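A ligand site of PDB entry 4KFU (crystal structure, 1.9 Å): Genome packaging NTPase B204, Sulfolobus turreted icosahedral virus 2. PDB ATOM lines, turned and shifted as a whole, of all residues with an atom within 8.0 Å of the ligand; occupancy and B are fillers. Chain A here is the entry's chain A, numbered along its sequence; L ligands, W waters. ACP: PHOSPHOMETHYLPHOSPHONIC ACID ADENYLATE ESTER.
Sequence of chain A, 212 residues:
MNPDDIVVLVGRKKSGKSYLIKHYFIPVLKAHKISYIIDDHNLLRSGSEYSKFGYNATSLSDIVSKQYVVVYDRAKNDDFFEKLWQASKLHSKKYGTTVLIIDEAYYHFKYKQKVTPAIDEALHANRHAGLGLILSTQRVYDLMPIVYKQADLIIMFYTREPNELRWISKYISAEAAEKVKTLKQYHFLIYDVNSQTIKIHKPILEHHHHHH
The backbone carbonyl oxygen (O) of Leu 183 lies within hydrogen-bond range of a nitrogen (N6) of the ligand.
The backbone carbonyl oxygen (O) of Lys 184 lies close to a nitrogen (N6) of the ligand, 3.4 Å away.
NZ of Lys 184 lies within salt-bridge range of O1A of the ligand (3.2 Å).
The backbone NH of Gln 185 lies close to a nitrogen (N6) of the ligand, 3.3 Å away.
Residues that only touch the ligand: Tyr 158.
Hydrophobic or aromatic side chains that line the ligand: Tyr 158.
Four residues have an atom within 4 Å of the ligand: Tyr 158, Leu 183, Lys 184 and Gln 185.
Water W2 lies within hydrogen-bond range of O of Leu 183 (2.9 Å), NZ of Lys 184 (3.0 Å) and N7 of the ligand (3.3 Å).
NE2 of Gln 185 lies within hydrogen-bond range of OH of Tyr 186, at 3.4 Å.
O of Gln 185 is in hydrogen-bond range of ND1 of His 187 (3.0 Å).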
ATOM      1  N   LYS A  14      17.116   4.829 -19.609  1.00  0.00           N
ATOM      2  CA  LYS A  14      17.622   4.133 -18.420  1.00  0.00           C
ATOM      3  C   LYS A  14      16.537   3.720 -17.417  1.00  0.00           C
ATOM      4  O   LYS A  14      16.865   3.292 -16.304  1.00  0.00           O
ATOM      5  CB  LYS A  14      18.724   4.936 -17.710  1.00  0.00           C
ATOM      6  CG  LYS A  14      19.822   5.475 -18.619  1.00  0.00           C
ATOM      7  CD  LYS A  14      20.640   4.355 -19.258  1.00  0.00           C
ATOM      8  CE  LYS A  14      21.658   4.919 -20.257  1.00  0.00           C
ATOM      9  NZ  LYS A  14      22.633   3.893 -20.714  1.00  0.00           N
ATOM     10  N   SER A  15      15.262   3.842 -17.792  1.00  0.00           N
ATOM     11  CA  SER A  15      14.163   3.375 -16.929  1.00  0.00           C
ATOM     12  C   SER A  15      14.145   1.857 -16.718  1.00  0.00           C
ATOM     13  O   SER A  15      13.679   1.379 -15.679  1.00  0.00           O
ATOM     14  CB  SER A  15      12.800   3.812 -17.472  1.00  0.00           C
ATOM     15  OG  SER A  15      12.574   3.245 -18.764  1.00  0.00           O
ATOM     16  N   PHE A 157       6.865   3.120 -16.781  1.00  0.00           N
ATOM     17  CA  PHE A 157       7.779   3.385 -15.662  1.00  0.00           C
ATOM     18  C   PHE A 157       7.521   4.797 -15.133  1.00  0.00           C
ATOM     19  O   PHE A 157       6.669   5.513 -15.671  1.00  0.00           O
ATOM     20  CB  PHE A 157       9.243   3.246 -16.091  1.00  0.00           C
ATOM     21  CG  PHE A 157       9.630   1.826 -16.443  1.00  0.00           C
ATOM     22  CD1 PHE A 157      10.358   1.054 -15.550  1.00  0.00           C
ATOM     23  CD2 PHE A 157       9.254   1.261 -17.654  1.00  0.00           C
ATOM     24  CE1 PHE A 157      10.720  -0.278 -15.860  1.00  0.00           C
ATOM     25  CE2 PHE A 157       9.619  -0.073 -17.977  1.00  0.00           C
ATOM     26  CZ  PHE A 157      10.350  -0.835 -17.071  1.00  0.00           C
ATOM     27  N   TYR A 158       8.256   5.199 -14.110  1.00  0.00           N
ATOM     28  CA  TYR A 158       8.032   6.462 -13.424  1.00  0.00           C
ATOM     29  C   TYR A 158       7.933   7.685 -14.342  1.00  0.00           C
ATOM     30  O   TYR A 158       8.781   7.873 -15.220  1.00  0.00           O
ATOM     31  CB  TYR A 158       9.136   6.710 -12.377  1.00  0.00           C
ATOM     32  CG  TYR A 158       9.201   8.150 -11.930  1.00  0.00           C
ATOM     33  CD1 TYR A 158       8.355   8.629 -10.918  1.00  0.00           C
ATOM     34  CD2 TYR A 158      10.098   9.050 -12.519  1.00  0.00           C
ATOM     35  CE1 TYR A 158       8.392   9.968 -10.514  1.00  0.00           C
ATOM     36  CE2 TYR A 158      10.145  10.394 -12.106  1.00  0.00           C
ATOM     37  CZ  TYR A 158       9.292  10.841 -11.113  1.00  0.00           C
ATOM     38  OH  TYR A 158       9.334  12.164 -10.728  1.00  0.00           O
ATOM     39  N   THR A 159       6.923   8.516 -14.119  1.00  0.00           N
ATOM     40  CA  THR A 159       6.954   9.889 -14.620  1.00  0.00           C
ATOM     41  C   THR A 159       6.054  10.814 -13.824  1.00  0.00           C
ATOM     42  O   THR A 159       5.026  10.391 -13.281  1.00  0.00           O
ATOM     43  CB  THR A 159       6.578   9.973 -16.116  1.00  0.00           C
ATOM     44  OG1 THR A 159       6.771  11.314 -16.561  1.00  0.00           O
ATOM     45  CG2 THR A 159       5.121   9.561 -16.342  1.00  0.00           C
ATOM     46  N   VAL A 180       1.476   6.174 -11.749  1.00  0.00           N
ATOM     47  CA  VAL A 180       2.795   6.219 -12.382  1.00  0.00           C
ATOM     48  C   VAL A 180       3.741   7.181 -11.643  1.00  0.00           C
ATOM     49  O   VAL A 180       4.982   7.037 -11.707  1.00  0.00           O
ATOM     50  CB  VAL A 180       2.662   6.597 -13.888  1.00  0.00           C
ATOM     51  CG1 VAL A 180       2.405   8.090 -14.066  1.00  0.00           C
ATOM     52  CG2 VAL A 180       3.895   6.184 -14.649  1.00  0.00           C
ATOM     53  N   LYS A 181       3.149   8.121 -10.901  1.00  0.00           N
ATOM     54  CA  LYS A 181       3.893   9.201 -10.251  1.00  0.00           C
ATOM     55  C   LYS A 181       4.743   8.724  -9.079  1.00  0.00           C
ATOM     56  O   LYS A 181       5.703   9.399  -8.690  1.00  0.00           O
ATOM     57  CB  LYS A 181       2.924  10.285  -9.744  1.00  0.00           C
ATOM     58  CG  LYS A 181       2.066  10.922 -10.823  1.00  0.00           C
ATOM     59  CD  LYS A 181       1.166  12.010 -10.245  1.00  0.00           C
ATOM     60  CE  LYS A 181       1.980  13.219  -9.803  1.00  0.00           C
ATOM     61  NZ  LYS A 181       1.120  14.385  -9.410  1.00  0.00           N
ATOM     62  N   THR A 182       4.400   7.576  -8.514  1.00  0.00           N
ATOM     63  CA  THR A 182       5.077   7.116  -7.304  1.00  0.00           C
ATOM     64  C   THR A 182       5.931   5.863  -7.498  1.00  0.00           C
ATOM     65  O   THR A 182       6.441   5.279  -6.533  1.00  0.00           O
ATOM     66  CB  THR A 182       4.049   6.893  -6.164  1.00  0.00           C
ATOM     67  OG1 THR A 182       3.009   6.044  -6.639  1.00  0.00           O
ATOM     68  CG2 THR A 182       3.452   8.236  -5.725  1.00  0.00           C
ATOM     69  N   LEU A 183       6.111   5.439  -8.748  1.00  0.00           N
ATOM     70  CA  LEU A 183       6.904   4.236  -9.011  1.00  0.00           C
ATOM     71  C   LEU A 183       8.370   4.442  -8.668  1.00  0.00           C
ATOM     72  O   LEU A 183       8.980   5.445  -9.069  1.00  0.00           O
ATOM     73  CB  LEU A 183       6.798   3.837 -10.478  1.00  0.00           C
ATOM     74  CG  LEU A 183       5.415   3.503 -11.014  1.00  0.00           C
ATOM     75  CD1 LEU A 183       5.433   3.499 -12.548  1.00  0.00           C
ATOM     76  CD2 LEU A 183       4.962   2.152 -10.455  1.00  0.00           C
ATOM     77  N   LYS A 184       8.955   3.473  -7.963  1.00  0.00           N
ATOM     78  CA  LYS A 184      10.382   3.525  -7.649  1.00  0.00           C
ATOM     79  C   LYS A 184      11.217   2.944  -8.795  1.00  0.00           C
ATOM     80  O   LYS A 184      10.669   2.481  -9.797  1.00  0.00           O
ATOM     81  CB  LYS A 184      10.672   2.816  -6.324  1.00  0.00           C
ATOM     82  CG  LYS A 184      10.116   3.552  -5.112  1.00  0.00           C
ATOM     83  CD  LYS A 184      10.312   5.063  -5.268  1.00  0.00           C
ATOM     84  CE  LYS A 184       9.639   5.849  -4.143  1.00  0.00           C
ATOM     85  NZ  LYS A 184       9.556   7.311  -4.459  1.00  0.00           N
ATOM     86  N   GLN A 185      12.539   3.012  -8.655  1.00  0.00           N
ATOM     87  CA  GLN A 185      13.421   2.604  -9.757  1.00  0.00           C
ATOM     88  C   GLN A 185      13.173   1.163 -10.201  1.00  0.00           C
ATOM     89  O   GLN A 185      13.106   0.246  -9.377  1.00  0.00           O
ATOM     90  CB  GLN A 185      14.902   2.789  -9.393  1.00  0.00           C
ATOM     91  CG  GLN A 185      15.829   2.600 -10.590  1.00  0.00           C
ATOM     92  CD  GLN A 185      17.267   3.036 -10.333  1.00  0.00           C
ATOM     93  OE1 GLN A 185      17.821   2.783  -9.261  1.00  0.00           O
ATOM     94  NE2 GLN A 185      17.865   3.692 -11.314  1.00  0.00           N
ATOM     95  N   TYR A 186      13.009   0.994 -11.514  1.00  0.00           N
ATOM     96  CA  TYR A 186      12.785  -0.312 -12.138  1.00  0.00           C
ATOM     97  C   TYR A 186      11.433  -0.959 -11.813  1.00  0.00           C
ATOM     98  O   TYR A 186      11.121  -2.028 -12.348  1.00  0.00           O
ATOM     99  CB  TYR A 186      13.925  -1.287 -11.817  1.00  0.00           C
ATOM    100  CG  TYR A 186      15.296  -0.722 -12.084  1.00  0.00           C
ATOM    101  CD1 TYR A 186      15.555  -0.019 -13.257  1.00  0.00           C
ATOM    102  CD2 TYR A 186      16.313  -0.883 -11.171  1.00  0.00           C
ATOM    103  CE1 TYR A 186      16.825   0.504 -13.508  1.00  0.00           C
ATOM    104  CE2 TYR A 186      17.587  -0.363 -11.413  1.00  0.00           C
ATOM    105  CZ  TYR A 186      17.828   0.328 -12.581  1.00  0.00           C
ATOM    106  OH  TYR A 186      19.074   0.855 -12.829  1.00  0.00           O
ATOM    107  N   HIS A 187      10.626  -0.294 -10.986  1.00  0.00           N
ATOM    108  CA  HIS A 187       9.246  -0.724 -10.775  1.00  0.00           C
ATOM    109  C   HIS A 187       8.429  -0.281 -11.987  1.00  0.00           C
ATOM    110  O   HIS A 187       8.748   0.739 -12.605  1.00  0.00           O
ATOM    111  CB  HIS A 187       8.645  -0.089  -9.514  1.00  0.00           C
ATOM    112  CG  HIS A 187       9.220  -0.613  -8.234  1.00  0.00           C
ATOM    113  ND1 HIS A 187      10.554  -0.501  -7.909  1.00  0.00           N
ATOM    114  CD2 HIS A 187       8.635  -1.252  -7.196  1.00  0.00           C
ATOM    115  CE1 HIS A 187      10.766  -1.055  -6.728  1.00  0.00           C
ATOM    116  NE2 HIS A 187       9.608  -1.516  -6.269  1.00  0.00           N
HETATM  117  PA  ACP L   1      13.387   6.930  -1.881  1.00  0.00           P
HETATM  118  O1A ACP L   1      11.984   7.085  -2.400  1.00  0.00           O
HETATM  119  O2A ACP L   1      13.791   7.645  -0.613  1.00  0.00           O
HETATM  120  O3A ACP L   1      13.706   5.350  -1.693  1.00  0.00           O
HETATM  121  O5' ACP L   1      14.399   7.352  -3.065  1.00  0.00           O
HETATM  122  C5' ACP L   1      15.805   7.511  -2.835  1.00  0.00           C
HETATM  123  C4' ACP L   1      16.457   7.817  -4.171  1.00  0.00           C
HETATM  124  O4' ACP L   1      15.877   6.994  -5.203  1.00  0.00           O
HETATM  125  C3' ACP L   1      16.233   9.261  -4.584  1.00  0.00           C
HETATM  126  O3' ACP L   1      17.479   9.807  -5.038  1.00  0.00           O
HETATM  127  C2' ACP L   1      15.340   9.194  -5.791  1.00  0.00           C
HETATM  128  O2' ACP L   1      15.682  10.229  -6.711  1.00  0.00           O
HETATM  129  C1' ACP L   1      15.645   7.811  -6.359  1.00  0.00           C
HETATM  130  N9  ACP L   1      14.477   7.323  -7.131  1.00  0.00           N
HETATM  131  C8  ACP L   1      13.208   7.290  -6.686  1.00  0.00           C
HETATM  132  N7  ACP L   1      12.372   6.811  -7.645  1.00  0.00           N
HETATM  133  C5  ACP L   1      13.124   6.546  -8.725  1.00  0.00           C
HETATM  134  C6  ACP L   1      12.877   6.026 -10.085  1.00  0.00           C
HETATM  135  N6  ACP L   1      11.624   5.682 -10.458  1.00  0.00           N
HETATM  136  N1  ACP L   1      13.943   5.897 -10.923  1.00  0.00           N
HETATM  137  C2  ACP L   1      15.196   6.240 -10.550  1.00  0.00           C
HETATM  138  N3  ACP L   1      15.486   6.718  -9.322  1.00  0.00           N
HETATM  139  C4  ACP L   1      14.519   6.892  -8.392  1.00  0.00           C
HETATM  140  O   HOH W   1      13.975   3.953  -6.284  1.00  0.00           O
HETATM  141  O   HOH W   2       9.270   7.820  -7.411  1.00  0.00           O
